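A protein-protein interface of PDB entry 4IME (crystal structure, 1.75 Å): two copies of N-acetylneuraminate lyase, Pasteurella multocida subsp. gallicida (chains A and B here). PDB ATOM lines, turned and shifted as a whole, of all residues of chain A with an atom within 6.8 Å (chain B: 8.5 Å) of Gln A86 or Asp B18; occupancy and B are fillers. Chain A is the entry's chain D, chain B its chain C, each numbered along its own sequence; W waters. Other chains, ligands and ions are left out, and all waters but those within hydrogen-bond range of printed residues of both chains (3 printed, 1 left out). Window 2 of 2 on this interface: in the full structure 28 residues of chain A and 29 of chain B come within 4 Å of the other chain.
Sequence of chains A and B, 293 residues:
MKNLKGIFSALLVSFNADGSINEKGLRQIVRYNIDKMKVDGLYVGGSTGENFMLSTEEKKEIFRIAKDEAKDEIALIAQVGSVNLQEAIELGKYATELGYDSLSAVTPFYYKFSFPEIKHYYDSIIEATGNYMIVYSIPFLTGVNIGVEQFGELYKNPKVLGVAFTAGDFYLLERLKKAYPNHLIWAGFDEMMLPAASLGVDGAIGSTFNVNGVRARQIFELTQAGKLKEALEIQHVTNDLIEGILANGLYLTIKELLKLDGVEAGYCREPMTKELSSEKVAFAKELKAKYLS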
ATOM      1  N   SER A  82      26.818 -27.228  34.952  1.00  0.00           N
ATOM      2  CA  SER A  82      26.813 -26.294  33.860  1.00  0.00           C
ATOM      3  C   SER A  82      25.808 -25.193  34.256  1.00  0.00           C
ATOM      4  O   SER A  82      24.998 -25.357  35.174  1.00  0.00           O
ATOM      5  CB  SER A  82      26.235 -27.085  32.661  1.00  0.00           C
ATOM      6  OG  SER A  82      25.926 -26.355  31.547  1.00  0.00           O
ATOM      7  N   VAL A  83      25.833 -24.091  33.521  1.00  0.00           N
ATOM      8  CA  VAL A  83      24.713 -23.148  33.597  1.00  0.00           C
ATOM      9  C   VAL A  83      23.448 -23.738  32.970  1.00  0.00           C
ATOM     10  O   VAL A  83      22.343 -23.327  33.309  1.00  0.00           O
ATOM     11  CB  VAL A  83      25.104 -21.829  32.896  1.00  0.00           C
ATOM     12  CG1 VAL A  83      24.053 -20.752  33.105  1.00  0.00           C
ATOM     13  CG2 VAL A  83      26.430 -21.273  33.425  1.00  0.00           C
ATOM     14  N   ASN A  84      23.624 -24.672  32.038  1.00  0.00           N
ATOM     15  CA  ASN A  84      22.507 -25.350  31.355  1.00  0.00           C
ATOM     16  C   ASN A  84      22.140 -26.613  32.129  1.00  0.00           C
ATOM     17  O   ASN A  84      22.808 -27.642  32.001  1.00  0.00           O
ATOM     18  CB  ASN A  84      22.983 -25.680  29.932  1.00  0.00           C
ATOM     19  CG  ASN A  84      21.917 -26.319  29.053  1.00  0.00           C
ATOM     20  OD1 ASN A  84      22.082 -26.432  27.794  1.00  0.00           O
ATOM     21  ND2 ASN A  84      20.842 -26.720  29.635  1.00  0.00           N
ATOM     22  N   LEU A  85      21.060 -26.533  32.915  1.00  0.00           N
ATOM     23  CA  LEU A  85      20.573 -27.677  33.687  1.00  0.00           C
ATOM     24  C   LEU A  85      20.120 -28.839  32.806  1.00  0.00           C
ATOM     25  O   LEU A  85      20.320 -29.991  33.180  1.00  0.00           O
ATOM     26  CB  LEU A  85      19.436 -27.258  34.638  1.00  0.00           C
ATOM     27  CG  LEU A  85      18.650 -28.361  35.366  1.00  0.00           C
ATOM     28  CD1 LEU A  85      19.562 -29.231  36.211  1.00  0.00           C
ATOM     29  CD2 LEU A  85      17.570 -27.720  36.241  1.00  0.00           C
ATOM     30  N   GLN A  86      19.528 -28.566  31.634  1.00  0.00           N
ATOM     31  CA  GLN A  86      19.097 -29.675  30.753  1.00  0.00           C
ATOM     32  C   GLN A  86      20.314 -30.443  30.186  1.00  0.00           C
ATOM     33  O   GLN A  86      20.258 -31.681  30.084  1.00  0.00           O
ATOM     34  CB  GLN A  86      18.083 -29.226  29.672  1.00  0.00           C
ATOM     35  CG  GLN A  86      16.935 -28.467  30.374  1.00  0.00           C
ATOM     36  CD  GLN A  86      15.711 -28.286  29.558  1.00  0.00           C
ATOM     37  OE1 GLN A  86      15.735 -28.427  28.345  1.00  0.00           O
ATOM     38  NE2 GLN A  86      14.608 -27.893  30.238  1.00  0.00           N
ATOM     39  N   GLU A  87      21.387 -29.718  29.865  1.00  0.00           N
ATOM     40  CA  GLU A  87      22.693 -30.357  29.549  1.00  0.00           C
ATOM     41  C   GLU A  87      23.229 -31.181  30.732  1.00  0.00           C
ATOM     42  O   GLU A  87      23.678 -32.313  30.559  1.00  0.00           O
ATOM     43  CB  GLU A  87      23.760 -29.323  29.133  1.00  0.00           C
ATOM     44  CG  GLU A  87      25.026 -30.019  28.657  1.00  0.00           C
ATOM     45  CD  GLU A  87      26.181 -29.076  28.475  1.00  0.00           C
ATOM     46  OE1 GLU A  87      26.254 -28.094  29.227  1.00  0.00           O
ATOM     47  OE2 GLU A  87      27.014 -29.289  27.577  1.00  0.00           O
ATOM     48  N   ALA A  88      23.147 -30.624  31.943  1.00  0.00           N
ATOM     49  CA  ALA A  88      23.629 -31.358  33.110  1.00  0.00           C
ATOM     50  C   ALA A  88      22.902 -32.689  33.293  1.00  0.00           C
ATOM     51  O   ALA A  88      23.534 -33.695  33.602  1.00  0.00           O
ATOM     52  CB  ALA A  88      23.537 -30.524  34.371  1.00  0.00           C
ATOM     53  N   ILE A  89      21.578 -32.663  33.138  1.00  0.00           N
ATOM     54  CA  ILE A  89      20.804 -33.878  33.226  1.00  0.00           C
ATOM     55  C   ILE A  89      21.195 -34.876  32.113  1.00  0.00           C
ATOM     56  O   ILE A  89      21.355 -36.079  32.371  1.00  0.00           O
ATOM     57  CB  ILE A  89      19.302 -33.550  33.142  1.00  0.00           C
ATOM     58  CG1 ILE A  89      18.849 -32.859  34.456  1.00  0.00           C
ATOM     59  CG2 ILE A  89      18.505 -34.827  32.936  1.00  0.00           C
ATOM     60  CD1 ILE A  89      17.458 -32.215  34.348  1.00  0.00           C
ATOM     61  N   GLU A  90      21.326 -34.390  30.878  1.00  0.00           N
ATOM     62  CA  GLU A  90      21.743 -35.268  29.743  1.00  0.00           C
ATOM     63  C   GLU A  90      23.091 -35.936  30.025  1.00  0.00           C
ATOM     64  O   GLU A  90      23.282 -37.126  29.791  1.00  0.00           O
ATOM     65  CB  GLU A  90      21.881 -34.443  28.456  1.00  0.00           C
ATOM     66  CG  GLU A  90      22.269 -35.233  27.201  1.00  0.00           C
ATOM     67  CD  GLU A  90      22.404 -34.346  25.944  1.00  0.00           C
ATOM     68  OE1 GLU A  90      22.862 -34.839  24.866  1.00  0.00           O
ATOM     69  OE2 GLU A  90      22.011 -33.156  26.003  1.00  0.00           O
ATOM     70  N   LEU A  91      24.068 -35.121  30.422  1.00  0.00           N
ATOM     71  CA  LEU A  91      25.389 -35.631  30.765  1.00  0.00           C
ATOM     72  C   LEU A  91      25.356 -36.564  31.980  1.00  0.00           C
ATOM     73  O   LEU A  91      26.067 -37.582  32.010  1.00  0.00           O
ATOM     74  CB  LEU A  91      26.368 -34.458  31.065  1.00  0.00           C
ATOM     75  CG  LEU A  91      26.728 -33.609  29.820  1.00  0.00           C
ATOM     76  CD1 LEU A  91      27.509 -32.351  30.249  1.00  0.00           C
ATOM     77  CD2 LEU A  91      27.492 -34.482  28.797  1.00  0.00           C
ATOM     78  N   PHE B  15       9.455 -19.199  26.896  1.00  0.00           N
ATOM     79  CA  PHE B  15       9.706 -20.636  27.103  1.00  0.00           C
ATOM     80  C   PHE B  15       8.432 -21.334  27.488  1.00  0.00           C
ATOM     81  O   PHE B  15       7.552 -20.753  28.131  1.00  0.00           O
ATOM     82  CB  PHE B  15      10.784 -20.879  28.186  1.00  0.00           C
ATOM     83  CG  PHE B  15      12.143 -20.379  27.773  1.00  0.00           C
ATOM     84  CD1 PHE B  15      12.635 -19.144  28.253  1.00  0.00           C
ATOM     85  CD2 PHE B  15      12.892 -21.111  26.877  1.00  0.00           C
ATOM     86  CE1 PHE B  15      13.887 -18.685  27.858  1.00  0.00           C
ATOM     87  CE2 PHE B  15      14.156 -20.659  26.432  1.00  0.00           C
ATOM     88  CZ  PHE B  15      14.656 -19.459  26.940  1.00  0.00           C
ATOM     89  N   ASN B  16       8.320 -22.586  27.055  1.00  0.00           N
ATOM     90  CA  ASN B  16       7.302 -23.495  27.583  1.00  0.00           C
ATOM     91  C   ASN B  16       7.700 -24.056  28.959  1.00  0.00           C
ATOM     92  O   ASN B  16       8.839 -23.854  29.400  1.00  0.00           O
ATOM     93  CB  ASN B  16       7.147 -24.651  26.600  1.00  0.00           C
ATOM     94  CG  ASN B  16       6.617 -24.191  25.264  1.00  0.00           C
ATOM     95  OD1 ASN B  16       5.589 -23.508  25.180  1.00  0.00           O
ATOM     96  ND2 ASN B  16       7.290 -24.585  24.198  1.00  0.00           N
ATOM     97  N   ALA B  17       6.777 -24.757  29.631  1.00  0.00           N
ATOM     98  CA  ALA B  17       7.084 -25.309  30.975  1.00  0.00           C
ATOM     99  C   ALA B  17       8.230 -26.327  30.943  1.00  0.00           C
ATOM    100  O   ALA B  17       8.934 -26.487  31.942  1.00  0.00           O
ATOM    101  CB  ALA B  17       5.847 -25.957  31.581  1.00  0.00           C
ATOM    102  N   ASP B  18       8.415 -27.019  29.806  1.00  0.00           N
ATOM    103  CA  ASP B  18       9.507 -27.978  29.697  1.00  0.00           C
ATOM    104  C   ASP B  18      10.828 -27.342  29.267  1.00  0.00           C
ATOM    105  O   ASP B  18      11.784 -28.060  28.995  1.00  0.00           O
ATOM    106  CB  ASP B  18       9.150 -29.126  28.743  1.00  0.00           C
ATOM    107  CG  ASP B  18       8.983 -28.675  27.312  1.00  0.00           C
ATOM    108  OD1 ASP B  18       9.159 -27.495  27.001  1.00  0.00           O
ATOM    109  OD2 ASP B  18       8.586 -29.514  26.470  1.00  0.00           O
ATOM    110  N   GLY B  19      10.889 -26.023  29.211  1.00  0.00           N
ATOM    111  CA  GLY B  19      12.141 -25.340  28.837  1.00  0.00           C
ATOM    112  C   GLY B  19      12.332 -25.144  27.362  1.00  0.00           C
ATOM    113  O   GLY B  19      13.248 -24.460  26.970  1.00  0.00           O
ATOM    114  N   SER B  20      11.472 -25.728  26.528  1.00  0.00           N
ATOM    115  CA  SER B  20      11.564 -25.492  25.092  1.00  0.00           C
ATOM    116  C   SER B  20      11.160 -24.077  24.717  1.00  0.00           C
ATOM    117  O   SER B  20      10.480 -23.373  25.501  1.00  0.00           O
ATOM    118  CB  SER B  20      10.770 -26.553  24.284  1.00  0.00           C
ATOM    119  OG  SER B  20       9.398 -26.505  24.602  1.00  0.00           O
ATOM    120  N   ILE B  21      11.560 -23.655  23.520  1.00  0.00           N
ATOM    121  CA  ILE B  21      11.169 -22.317  23.063  1.00  0.00           C
ATOM    122  C   ILE B  21       9.730 -22.334  22.563  1.00  0.00           C
ATOM    123  O   ILE B  21       9.390 -23.171  21.727  1.00  0.00           O
ATOM    124  CB  ILE B  21      12.071 -21.839  21.901  1.00  0.00           C
ATOM    125  CG1 ILE B  21      13.528 -21.626  22.396  1.00  0.00           C
ATOM    126  CG2 ILE B  21      11.532 -20.526  21.330  1.00  0.00           C
ATOM    127  CD1 ILE B  21      14.513 -22.080  21.310  1.00  0.00           C
ATOM    128  N   ASN B  22       8.888 -21.444  23.078  1.00  0.00           N
ATOM    129  CA  ASN B  22       7.544 -21.253  22.498  1.00  0.00           C
ATOM    130  C   ASN B  22       7.626 -20.268  21.327  1.00  0.00           C
ATOM    131  O   ASN B  22       7.672 -19.045  21.533  1.00  0.00           O
ATOM    132  CB  ASN B  22       6.527 -20.796  23.544  1.00  0.00           C
ATOM    133  CG  ASN B  22       5.102 -20.821  23.002  1.00  0.00           C
ATOM    134  OD1 ASN B  22       4.331 -21.766  23.229  1.00  0.00           O
ATOM    135  ND2 ASN B  22       4.758 -19.799  22.257  1.00  0.00           N
ATOM    136  N   MET B  53      21.833 -20.488  29.554  1.00  0.00           N
ATOM    137  CA  MET B  53      21.250 -21.723  30.037  1.00  0.00           C
ATOM    138  C   MET B  53      20.813 -22.690  28.910  1.00  0.00           C
ATOM    139  O   MET B  53      20.271 -23.779  29.211  1.00  0.00           O
ATOM    140  CB  MET B  53      19.994 -21.405  30.915  1.00  0.00           C
ATOM    141  CG  MET B  53      20.412 -20.664  32.208  1.00  0.00           C
ATOM    142  SD  MET B  53      18.943 -20.318  33.236  1.00  0.00           S
ATOM    143  CE  MET B  53      18.120 -19.140  32.188  1.00  0.00           C
ATOM    144  N   LEU B  54      21.072 -22.292  27.662  1.00  0.00           N
ATOM    145  CA  LEU B  54      20.527 -22.999  26.473  1.00  0.00           C
ATOM    146  C   LEU B  54      21.547 -23.831  25.722  1.00  0.00           C
ATOM    147  O   LEU B  54      22.765 -23.592  25.827  1.00  0.00           O
ATOM    148  CB  LEU B  54      19.918 -21.984  25.488  1.00  0.00           C
ATOM    149  CG  LEU B  54      18.908 -20.983  26.074  1.00  0.00           C
ATOM    150  CD1 LEU B  54      18.273 -20.139  24.968  1.00  0.00           C
ATOM    151  CD2 LEU B  54      17.803 -21.689  26.887  1.00  0.00           C
ATOM    152  N   SER B  55      21.035 -24.791  24.952  1.00  0.00           N
ATOM    153  CA  SER B  55      21.840 -25.592  23.999  1.00  0.00           C
ATOM    154  C   SER B  55      22.171 -24.807  22.719  1.00  0.00           C
ATOM    155  O   SER B  55      21.536 -23.799  22.411  1.00  0.00           O
ATOM    156  CB  SER B  55      21.106 -26.855  23.643  1.00  0.00           C
ATOM    157  OG  SER B  55      20.054 -26.576  22.685  1.00  0.00           O
ATOM    158  N   GLU B  58      19.243 -24.671  20.484  1.00  0.00           N
ATOM    159  CA  GLU B  58      18.257 -23.700  20.955  1.00  0.00           C
ATOM    160  C   GLU B  58      18.675 -22.288  20.589  1.00  0.00           C
ATOM    161  O   GLU B  58      17.825 -21.490  20.176  1.00  0.00           O
ATOM    162  CB  GLU B  58      18.010 -23.808  22.475  1.00  0.00           C
ATOM    163  CG  GLU B  58      17.134 -25.012  22.826  1.00  0.00           C
ATOM    164  CD  GLU B  58      17.295 -25.557  24.261  1.00  0.00           C
ATOM    165  OE1 GLU B  58      18.241 -25.197  25.001  1.00  0.00           O
ATOM    166  OE2 GLU B  58      16.447 -26.410  24.633  1.00  0.00           O
ATOM    167  N   TYR B 267       7.269 -18.800  30.230  1.00  0.00           N
ATOM    168  CA  TYR B 267       7.933 -19.124  31.488  1.00  0.00           C
ATOM    169  C   TYR B 267       9.367 -18.669  31.323  1.00  0.00           C
ATOM    170  O   TYR B 267       9.829 -18.398  30.210  1.00  0.00           O
ATOM    171  CB  TYR B 267       7.941 -20.647  31.712  1.00  0.00           C
ATOM    172  CG  TYR B 267       6.563 -21.254  31.972  1.00  0.00           C
ATOM    173  CD1 TYR B 267       5.740 -21.624  30.935  1.00  0.00           C
ATOM    174  CD2 TYR B 267       6.111 -21.438  33.282  1.00  0.00           C
ATOM    175  CE1 TYR B 267       4.457 -22.149  31.184  1.00  0.00           C
ATOM    176  CE2 TYR B 267       4.859 -22.010  33.533  1.00  0.00           C
ATOM    177  CZ  TYR B 267       4.048 -22.344  32.484  1.00  0.00           C
ATOM    178  OH  TYR B 267       2.808 -22.898  32.776  1.00  0.00           O
ATOM    179  N   CYS B 268      10.076 -18.640  32.453  1.00  0.00           N
ATOM    180  CA  CYS B 268      11.545 -18.629  32.388  1.00  0.00           C
ATOM    181  C   CYS B 268      12.097 -20.049  32.333  1.00  0.00           C
ATOM    182  O   CYS B 268      11.413 -21.038  32.604  1.00  0.00           O
ATOM    183  CB  CYS B 268      12.165 -17.891  33.591  1.00  0.00           C
ATOM    184  SG  CYS B 268      12.101 -16.099  33.411  1.00  0.00           S
ATOM    185  N   ARG B 269      13.362 -20.143  31.973  1.00  0.00           N
ATOM    186  CA  ARG B 269      14.036 -21.414  31.735  1.00  0.00           C
ATOM    187  C   ARG B 269      14.796 -21.860  32.991  1.00  0.00           C
ATOM    188  O   ARG B 269      15.559 -21.077  33.562  1.00  0.00           O
ATOM    189  CB  ARG B 269      15.029 -21.181  30.593  1.00  0.00           C
ATOM    190  CG  ARG B 269      16.084 -22.265  30.395  1.00  0.00           C
ATOM    191  CD  ARG B 269      15.534 -23.545  29.786  1.00  0.00           C
ATOM    192  NE  ARG B 269      16.680 -24.398  29.437  1.00  0.00           N
ATOM    193  CZ  ARG B 269      16.906 -24.976  28.263  1.00  0.00           C
ATOM    194  NH1 ARG B 269      15.968 -24.960  27.292  1.00  0.00           N
ATOM    195  NH2 ARG B 269      18.060 -25.637  28.082  1.00  0.00           N
ATOM    196  N   GLU B 270      14.597 -23.114  33.417  1.00  0.00           N
ATOM    197  CA  GLU B 270      15.321 -23.633  34.590  1.00  0.00           C
ATOM    198  C   GLU B 270      16.818 -23.600  34.226  1.00  0.00           C
ATOM    199  O   GLU B 270      17.193 -23.826  33.073  1.00  0.00           O
ATOM    200  CB  GLU B 270      14.839 -25.049  34.930  1.00  0.00           C
ATOM    201  CG  GLU B 270      15.178 -26.081  33.843  1.00  0.00           C
ATOM    202  CD  GLU B 270      14.649 -27.496  34.120  1.00  0.00           C
ATOM    203  OE1 GLU B 270      14.761 -28.345  33.201  1.00  0.00           O
ATOM    204  OE2 GLU B 270      14.106 -27.787  35.229  1.00  0.00           O
ATOM    205  N   PRO B 271      17.708 -23.363  35.202  1.00  0.00           N
ATOM    206  CA  PRO B 271      17.466 -23.345  36.634  1.00  0.00           C
ATOM    207  C   PRO B 271      16.932 -22.022  37.207  1.00  0.00           C
ATOM    208  O   PRO B 271      16.826 -21.893  38.441  1.00  0.00           O
ATOM    209  CB  PRO B 271      18.862 -23.674  37.228  1.00  0.00           C
ATOM    210  CG  PRO B 271      19.820 -23.230  36.212  1.00  0.00           C
ATOM    211  CD  PRO B 271      19.139 -23.513  34.880  1.00  0.00           C
ATOM    212  N   LYS B 274      10.731 -20.672  37.280  1.00  0.00           N
ATOM    213  CA  LYS B 274      10.050 -20.599  35.997  1.00  0.00           C
ATOM    214  C   LYS B 274       8.813 -19.774  35.923  1.00  0.00           C
ATOM    215  O   LYS B 274       8.406 -19.384  34.824  1.00  0.00           O
ATOM    216  CB  LYS B 274       9.835 -21.977  35.342  1.00  0.00           C
ATOM    217  CG  LYS B 274       9.350 -23.128  36.142  1.00  0.00           C
ATOM    218  CD  LYS B 274       9.759 -24.363  35.328  1.00  0.00           C
ATOM    219  CE  LYS B 274       8.584 -25.297  35.172  1.00  0.00           C
ATOM    220  NZ  LYS B 274       9.049 -26.642  34.718  1.00  0.00           N
HETATM  221  O   HOH W   1      24.622 -26.413  26.523  1.00  0.00           O
HETATM  222  O   HOH W   2      17.493 -28.286  26.275  1.00  0.00           O
HETATM  223  O   HOH W   3      13.524 -28.569  26.891  1.00  0.00           O
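Of the 18 printed residues of chain B, 8 touch a printed residue of chain A.
Hydrophobic or aromatic side chains of chain B within 4 Å of the printed part of chain A: Met B53 and Pro B271.
Water W3 lies within hydrogen-bond range of OE1 of Gln A86 (2.7 Å) and O of Asp B18 (2.8 Å).
Water W2 lies within hydrogen-bond range of the side-chain carboxylate (OE2) of Glu B58, the side-chain amide oxygen (OE1) of Gln A86 and the guanidinium group (NH2) of Arg B269.
Water W1 lies within hydrogen-bond range of the side-chain amide oxygen (OD1) of Asn A84 (2.8 Å) and the backbone carbonyl oxygen (O) of Leu B54 (3.4 Å).
No position is printed for both chains.
Among the printed residues, merely in contact across the chains: Val A83 with Met B53 (3.5 Å), Val A83 with Pro B271 (3.6 Å), Asn A84 with Leu B54 (3.4 Å), Leu A85 with Glu B270 (3.6 Å), Leu A85 with Pro B271 (3.8 Å), Gln A86 with Gly B19 (3.8 Å) and Gln A86 with Arg B269 (3.6 Å).
The side-chain carboxylate (OE2) of Glu B58 lies within salt-bridge range of the guanidinium group (NH1) of Arg B269, at 3.1 Å.
OG of Ser A82 is in hydrogen-bond range of N of Asn A84.
The side-chain carboxylate (OE1) of Glu B58 sits at hydrogen-bond distance from the backbone NH (N) of Ser B55 (2.8 Å).
O of Gly B19 lies within hydrogen-bond range of NH1 of Arg B269, 2.8 Å away.
The backbone carbonyl oxygen (O) of Met B53 lies within hydrogen-bond range of the guanidinium group (NH2) of Arg B269.
OG of Ser B20 sits at hydrogen-bond distance from OD1 of Asp B18.
Of chain A, only Gln A86 (3.1 Å) comes within 4 Å of Asp B18.
Of the printed residues of chain A, Gly B19 touches Gln A86.
Of the printed residues of chain A, Pro B271 touches Val A83 and Leu A85.
Printed residues of chain A within 4 Å of Leu B54: Asn A84.
The nearest printed residue of chain A that does not touch Asp B18 is Ile A89 (8.8 Å).
The nearest printed residue of chain A that does not touch Met B53 is Leu A85 (4.7 Å).
The guanidinium group of Arg B269 lies close to the side-chain amide nitrogen of Asn A84 (3.4 Å).
NE2 of Gln A86 is in hydrogen-bond range of OE1 of Glu B270, at 3.0 Å.
The backbone carbonyl oxygen (O) of Met B53 lies within hydrogen-bond range of the side-chain amide nitrogen (ND2) of Asn A84 (3.0 Å).
N of Ser B55 lies within hydrogen-bond range of OD1 of Asn A84.
The side-chain amide nitrogen (NE2) of Gln A86 sits at hydrogen-bond distance from the backbone carbonyl oxygen (O) of Asp B18 (3.1 Å).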
